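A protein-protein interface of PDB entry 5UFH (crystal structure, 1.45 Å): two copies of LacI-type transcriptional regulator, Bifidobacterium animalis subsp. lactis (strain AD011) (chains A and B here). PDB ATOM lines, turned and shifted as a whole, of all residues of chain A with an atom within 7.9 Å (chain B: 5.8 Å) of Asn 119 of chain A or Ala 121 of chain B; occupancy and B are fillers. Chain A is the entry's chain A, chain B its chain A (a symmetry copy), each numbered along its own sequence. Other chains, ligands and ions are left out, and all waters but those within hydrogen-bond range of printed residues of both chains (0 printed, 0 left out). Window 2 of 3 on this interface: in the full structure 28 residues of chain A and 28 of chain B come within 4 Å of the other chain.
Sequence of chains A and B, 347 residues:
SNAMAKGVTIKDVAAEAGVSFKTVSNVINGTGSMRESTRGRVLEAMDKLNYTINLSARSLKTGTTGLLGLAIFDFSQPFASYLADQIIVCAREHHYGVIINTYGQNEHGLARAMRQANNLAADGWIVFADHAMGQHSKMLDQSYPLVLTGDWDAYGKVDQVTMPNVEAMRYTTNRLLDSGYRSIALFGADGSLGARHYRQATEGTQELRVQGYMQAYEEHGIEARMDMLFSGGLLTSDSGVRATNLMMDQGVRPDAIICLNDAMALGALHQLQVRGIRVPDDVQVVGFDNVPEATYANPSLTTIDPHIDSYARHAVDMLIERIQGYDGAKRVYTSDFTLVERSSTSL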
ATOM      1  N   ILE A  99      -0.285 -26.425  -5.074  1.00  0.00           N
ATOM      2  CA  ILE A  99       0.202 -26.073  -3.742  1.00  0.00           C
ATOM      3  C   ILE A  99      -0.886 -26.412  -2.744  1.00  0.00           C
ATOM      4  O   ILE A  99      -2.077 -26.280  -3.036  1.00  0.00           O
ATOM      5  CB  ILE A  99       0.589 -24.589  -3.615  1.00  0.00           C
ATOM      6  CG1 ILE A  99      -0.610 -23.700  -3.958  1.00  0.00           C
ATOM      7  CG2 ILE A  99       1.742 -24.286  -4.509  1.00  0.00           C
ATOM      8  CD1 ILE A  99      -0.452 -22.318  -3.538  1.00  0.00           C
ATOM      9  N   ALA A 113      -8.067 -19.746   5.677  1.00  0.00           N
ATOM     10  CA  ALA A 113      -7.458 -20.265   4.454  1.00  0.00           C
ATOM     11  C   ALA A 113      -8.077 -19.649   3.195  1.00  0.00           C
ATOM     12  O   ALA A 113      -7.355 -19.332   2.240  1.00  0.00           O
ATOM     13  CB  ALA A 113      -7.572 -21.786   4.412  1.00  0.00           C
ATOM     14  N   MET A 114      -9.405 -19.482   3.164  1.00  0.00           N
ATOM     15  CA  MET A 114     -10.074 -18.840   2.016  1.00  0.00           C
ATOM     16  C   MET A 114      -9.571 -17.401   1.847  1.00  0.00           C
ATOM     17  O   MET A 114      -9.457 -16.906   0.732  1.00  0.00           O
ATOM     18  CB  MET A 114     -11.591 -18.773   2.192  1.00  0.00           C
ATOM     19  CG  MET A 114     -12.256 -19.972   2.785  1.00  0.00           C
ATOM     20  SD  MET A 114     -12.843 -21.324   1.515  1.00  0.00           S
ATOM     21  CE  MET A 114     -12.651 -20.386  -0.158  1.00  0.00           C
ATOM     22  N   ARG A 115      -9.280 -16.728   2.958  1.00  0.00           N
ATOM     23  CA  ARG A 115      -8.728 -15.384   2.857  1.00  0.00           C
ATOM     24  C   ARG A 115      -7.273 -15.422   2.413  1.00  0.00           C
ATOM     25  O   ARG A 115      -6.862 -14.624   1.565  1.00  0.00           O
ATOM     26  CB  ARG A 115      -8.891 -14.634   4.179  1.00  0.00           C
ATOM     27  CG  ARG A 115     -10.327 -14.503   4.642  1.00  0.00           C
ATOM     28  CD  ARG A 115     -10.438 -13.559   5.835  1.00  0.00           C
ATOM     29  NE  ARG A 115      -9.704 -14.040   7.005  1.00  0.00           N
ATOM     30  CZ  ARG A 115     -10.269 -14.656   8.039  1.00  0.00           C
ATOM     31  NH1 ARG A 115     -11.580 -14.870   8.049  1.00  0.00           N
ATOM     32  NH2 ARG A 115      -9.523 -15.053   9.060  1.00  0.00           N
ATOM     33  N   GLN A 116      -6.481 -16.348   2.966  1.00  0.00           N
ATOM     34  CA  GLN A 116      -5.075 -16.457   2.582  1.00  0.00           C
ATOM     35  C   GLN A 116      -4.916 -16.715   1.093  1.00  0.00           C
ATOM     36  O   GLN A 116      -3.922 -16.280   0.495  1.00  0.00           O
ATOM     37  CB  GLN A 116      -4.405 -17.595   3.357  1.00  0.00           C
ATOM     38  CG  GLN A 116      -4.165 -17.316   4.821  1.00  0.00           C
ATOM     39  CD  GLN A 116      -3.772 -18.566   5.587  1.00  0.00           C
ATOM     40  OE1 GLN A 116      -3.866 -19.679   5.073  1.00  0.00           O
ATOM     41  NE2 GLN A 116      -3.345 -18.383   6.830  1.00  0.00           N
ATOM     42  N   ALA A 117      -5.882 -17.413   0.486  1.00  0.00           N
ATOM     43  CA  ALA A 117      -5.820 -17.738  -0.933  1.00  0.00           C
ATOM     44  C   ALA A 117      -5.711 -16.487  -1.796  1.00  0.00           C
ATOM     45  O   ALA A 117      -5.151 -16.544  -2.895  1.00  0.00           O
ATOM     46  CB  ALA A 117      -7.065 -18.533  -1.335  1.00  0.00           C
ATOM     47  N   ASN A 118      -6.246 -15.354  -1.325  1.00  0.00           N
ATOM     48  CA  ASN A 118      -6.151 -14.112  -2.088  1.00  0.00           C
ATOM     49  C   ASN A 118      -4.707 -13.687  -2.333  1.00  0.00           C
ATOM     50  O   ASN A 118      -4.423 -13.020  -3.332  1.00  0.00           O
ATOM     51  CB  ASN A 118      -6.895 -12.987  -1.372  1.00  0.00           C
ATOM     52  CG  ASN A 118      -8.400 -13.195  -1.355  1.00  0.00           C
ATOM     53  OD1 ASN A 118      -9.039 -13.059  -0.312  1.00  0.00           O
ATOM     54  ND2 ASN A 118      -8.975 -13.517  -2.509  1.00  0.00           N
ATOM     55  N   ASN A 119      -3.786 -14.053  -1.442  1.00  0.00           N
ATOM     56  CA  ASN A 119      -2.405 -13.591  -1.508  1.00  0.00           C
ATOM     57  C   ASN A 119      -1.430 -14.703  -1.863  1.00  0.00           C
ATOM     58  O   ASN A 119      -0.209 -14.488  -1.835  1.00  0.00           O
ATOM     59  CB  ASN A 119      -2.026 -12.919  -0.192  1.00  0.00           C
ATOM     60  CG  ASN A 119      -3.013 -11.828   0.205  1.00  0.00           C
ATOM     61  OD1 ASN A 119      -3.611 -11.885   1.283  1.00  0.00           O
ATOM     62  ND2 ASN A 119      -3.198 -10.835  -0.672  1.00  0.00           N
ATOM     63  N   LEU A 120      -1.939 -15.892  -2.189  1.00  0.00           N
ATOM     64  CA  LEU A 120      -1.107 -16.968  -2.683  1.00  0.00           C
ATOM     65  C   LEU A 120      -1.062 -16.909  -4.211  1.00  0.00           C
ATOM     66  O   LEU A 120      -1.764 -16.124  -4.853  1.00  0.00           O
ATOM     67  CB  LEU A 120      -1.579 -18.316  -2.126  1.00  0.00           C
ATOM     68  CG  LEU A 120      -1.446 -18.523  -0.599  1.00  0.00           C
ATOM     69  CD1 LEU A 120      -2.018 -19.859  -0.191  1.00  0.00           C
ATOM     70  CD2 LEU A 120       0.001 -18.462  -0.075  1.00  0.00           C
ATOM     71  N   ALA A 121      -0.238 -17.760  -4.807  1.00  0.00           N
ATOM     72  CA  ALA A 121       0.021 -17.644  -6.234  1.00  0.00           C
ATOM     73  C   ALA A 121      -0.929 -18.476  -7.083  1.00  0.00           C
ATOM     74  O   ALA A 121      -0.993 -18.268  -8.296  1.00  0.00           O
ATOM     75  CB  ALA A 121       1.477 -18.026  -6.536  1.00  0.00           C
ATOM     76  N   ALA A 122      -1.685 -19.377  -6.470  1.00  0.00           N
ATOM     77  CA  ALA A 122      -2.531 -20.292  -7.230  1.00  0.00           C
ATOM     78  C   ALA A 122      -3.613 -19.549  -8.019  1.00  0.00           C
ATOM     79  O   ALA A 122      -4.131 -18.511  -7.599  1.00  0.00           O
ATOM     80  CB  ALA A 122      -3.175 -21.317  -6.295  1.00  0.00           C
ATOM     81  N   TRP A 125      -8.754 -22.644  -6.569  1.00  0.00           N
ATOM     82  CA  TRP A 125      -8.693 -23.471  -5.370  1.00  0.00           C
ATOM     83  C   TRP A 125      -9.707 -24.594  -5.400  1.00  0.00           C
ATOM     84  O   TRP A 125     -10.871 -24.400  -5.779  1.00  0.00           O
ATOM     85  CB  TRP A 125      -8.881 -22.636  -4.082  1.00  0.00           C
ATOM     86  CG  TRP A 125      -7.646 -21.852  -3.853  1.00  0.00           C
ATOM     87  CD1 TRP A 125      -7.299 -20.662  -4.435  1.00  0.00           C
ATOM     88  CD2 TRP A 125      -6.533 -22.249  -3.043  1.00  0.00           C
ATOM     89  NE1 TRP A 125      -6.030 -20.293  -4.011  1.00  0.00           N
ATOM     90  CE2 TRP A 125      -5.542 -21.250  -3.158  1.00  0.00           C
ATOM     91  CE3 TRP A 125      -6.290 -23.353  -2.221  1.00  0.00           C
ATOM     92  CZ2 TRP A 125      -4.309 -21.316  -2.465  1.00  0.00           C
ATOM     93  CZ3 TRP A 125      -5.060 -23.429  -1.543  1.00  0.00           C
ATOM     94  CH2 TRP A 125      -4.093 -22.412  -1.686  1.00  0.00           C
ATOM     95  N   TYR A 144     -11.589 -15.623  -6.658  1.00  0.00           N
ATOM     96  CA  TYR A 144     -10.836 -16.566  -7.456  1.00  0.00           C
ATOM     97  C   TYR A 144     -11.705 -17.775  -7.777  1.00  0.00           C
ATOM     98  O   TYR A 144     -12.663 -18.068  -7.053  1.00  0.00           O
ATOM     99  CB  TYR A 144      -9.596 -17.021  -6.674  1.00  0.00           C
ATOM    100  CG  TYR A 144      -9.873 -17.386  -5.233  1.00  0.00           C
ATOM    101  CD1 TYR A 144     -10.368 -18.645  -4.897  1.00  0.00           C
ATOM    102  CD2 TYR A 144      -9.639 -16.473  -4.209  1.00  0.00           C
ATOM    103  CE1 TYR A 144     -10.630 -18.979  -3.582  1.00  0.00           C
ATOM    104  CE2 TYR A 144      -9.894 -16.804  -2.885  1.00  0.00           C
ATOM    105  CZ  TYR A 144     -10.394 -18.060  -2.583  1.00  0.00           C
ATOM    106  OH  TYR A 144     -10.639 -18.388  -1.271  1.00  0.00           O
ATOM    107  N   LEU B  67       4.896 -17.023   6.749  1.00  0.00           N
ATOM    108  CA  LEU B  67       4.483 -18.177   5.960  1.00  0.00           C
ATOM    109  C   LEU B  67       5.702 -19.007   5.596  1.00  0.00           C
ATOM    110  O   LEU B  67       6.617 -18.499   4.943  1.00  0.00           O
ATOM    111  CB  LEU B  67       3.790 -17.699   4.693  1.00  0.00           C
ATOM    112  CG  LEU B  67       3.482 -18.855   3.770  1.00  0.00           C
ATOM    113  CD1 LEU B  67       2.569 -19.824   4.484  1.00  0.00           C
ATOM    114  CD2 LEU B  67       2.872 -18.309   2.472  1.00  0.00           C
ATOM    115  N   ILE B  99       2.679 -23.627   3.671  1.00  0.00           N
ATOM    116  CA  ILE B  99       2.176 -24.100   2.383  1.00  0.00           C
ATOM    117  C   ILE B  99       3.077 -25.225   1.916  1.00  0.00           C
ATOM    118  O   ILE B  99       4.288 -25.207   2.155  1.00  0.00           O
ATOM    119  CB  ILE B  99       2.120 -22.993   1.315  1.00  0.00           C
ATOM    120  CG1 ILE B  99       3.511 -22.384   1.114  1.00  0.00           C
ATOM    121  CG2 ILE B  99       1.140 -21.947   1.719  1.00  0.00           C
ATOM    122  CD1 ILE B  99       3.630 -21.590  -0.097  1.00  0.00           C
ATOM    123  N   ALA B 117       9.672 -21.704  -5.861  1.00  0.00           N
ATOM    124  CA  ALA B 117       9.655 -21.034  -4.568  1.00  0.00           C
ATOM    125  C   ALA B 117       9.896 -19.536  -4.704  1.00  0.00           C
ATOM    126  O   ALA B 117       9.428 -18.758  -3.866  1.00  0.00           O
ATOM    127  CB  ALA B 117      10.719 -21.646  -3.655  1.00  0.00           C
ATOM    128  N   ASN B 119       8.538 -17.526  -6.672  1.00  0.00           N
ATOM    129  CA  ASN B 119       7.304 -16.834  -7.025  1.00  0.00           C
ATOM    130  C   ASN B 119       6.139 -17.218  -6.126  1.00  0.00           C
ATOM    131  O   ASN B 119       4.998 -16.805  -6.383  1.00  0.00           O
ATOM    132  CB  ASN B 119       6.980 -17.085  -8.494  1.00  0.00           C
ATOM    133  CG  ASN B 119       8.149 -16.746  -9.411  1.00  0.00           C
ATOM    134  OD1 ASN B 119       8.630 -17.603 -10.156  1.00  0.00           O
ATOM    135  ND2 ASN B 119       8.621 -15.496  -9.348  1.00  0.00           N
ATOM    136  N   LEU B 120       6.395 -18.007  -5.083  1.00  0.00           N
ATOM    137  CA  LEU B 120       5.387 -18.308  -4.088  1.00  0.00           C
ATOM    138  C   LEU B 120       5.480 -17.286  -2.952  1.00  0.00           C
ATOM    139  O   LEU B 120       6.389 -16.455  -2.898  1.00  0.00           O
ATOM    140  CB  LEU B 120       5.502 -19.765  -3.625  1.00  0.00           C
ATOM    141  CG  LEU B 120       5.203 -20.855  -4.682  1.00  0.00           C
ATOM    142  CD1 LEU B 120       5.429 -22.231  -4.105  1.00  0.00           C
ATOM    143  CD2 LEU B 120       3.768 -20.819  -5.241  1.00  0.00           C
ATOM    144  N   ALA B 121       4.538 -17.357  -2.021  1.00  0.00           N
ATOM    145  CA  ALA B 121       4.428 -16.311  -1.016  1.00  0.00           C
ATOM    146  C   ALA B 121       5.235 -16.602   0.240  1.00  0.00           C
ATOM    147  O   ALA B 121       5.441 -15.695   1.048  1.00  0.00           O
ATOM    148  CB  ALA B 121       2.953 -16.080  -0.660  1.00  0.00           C
ATOM    149  N   ALA B 122       5.719 -17.827   0.400  1.00  0.00           N
ATOM    150  CA  ALA B 122       6.400 -18.213   1.632  1.00  0.00           C
ATOM    151  C   ALA B 122       7.679 -17.403   1.857  1.00  0.00           C
ATOM    152  O   ALA B 122       8.380 -17.015   0.919  1.00  0.00           O
ATOM    153  CB  ALA B 122       6.721 -19.708   1.612  1.00  0.00           C
ATOM    154  N   ASP B 123       7.986 -17.164   3.136  1.00  0.00           N
ATOM    155  CA  ASP B 123       9.157 -16.391   3.545  1.00  0.00           C
ATOM    156  C   ASP B 123      10.433 -17.214   3.573  1.00  0.00           C
ATOM    157  O   ASP B 123      11.520 -16.639   3.727  1.00  0.00           O
ATOM    158  CB  ASP B 123       8.922 -15.777   4.933  1.00  0.00           C
ATOM    159  CG  ASP B 123       7.781 -14.778   4.941  1.00  0.00           C
ATOM    160  OD1 ASP B 123       7.730 -13.956   4.011  1.00  0.00           O
ATOM    161  OD2 ASP B 123       6.943 -14.818   5.865  1.00  0.00           O
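The backbone carbonyl oxygen of Leu 67 of chain B sits at hydrogen-bond distance from the backbone NH of Asp 123 of chain B (2.6 Å).
Among the printed residues, pairs that only touch across the chains: Ala 121 of chain A with Asn 119 of chain B, Asn 119 of chain A with Ala 121 of chain B, Ala 121 of chain A with Leu 120 of chain B, Leu 120 of chain A with Ala 121 of chain B and Leu 120 of chain A with Leu 67 of chain B.
Of chain B, only Ala 121 comes within 4 Å of Asn 119 of chain A. Of the printed residues of chain B, Leu 120 of chain A touches Leu 67 (3.8 Å) and Ala 121 (3.8 Å). Of the printed residues of chain B, Ala 121 of chain A touches Asn 119 (3.7 Å) and Leu 120 (3.8 Å). Printed residues of chain A within 4 Å of Leu 67 of chain B: Leu 120 (3.8 Å). Of the printed residues of chain A, Leu 120 of chain B touches Ala 121. Of chain A, only Asn 119 and Leu 120 come within 4 Å of Ala 121 of chain B. No residue of chain A comes within 4 Å of Ala 122 of chain B. The nearest printed residue of chain B that does not touch Ala 121 of chain A is Ala 121 of chain B (5.5 Å).
Printed residues of chain B that touch a printed residue of chain A: Leu 67, Asn 119, Leu 120 and Ala 121. Hydrophobic or aromatic side chains of chain B that line the printed part of chain A: Leu 67, Leu 120 and Ala 121. Of the 13 printed residues of chain A, 3 touch a printed residue of chain B. Along chain A the printed residues that touch a printed residue of chain B span positions 119 to 121. Among the printed residues, 5 pairs touch across the chains.
Asn 119 of chain A touches Ala 121 of chain B, and with the chains exchanged Ala 121 of chain A touches Asn 119 of chain B. Leu 120 of chain A touches Ala 121 of chain B, and with the chains exchanged Ala 121 of chain A touches Leu 120 of chain B. 6 positions are printed for both chains. Of the 5 pairs that touch across the chains among the printed residues, 4 have their exchanged pair printed and touching as well.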
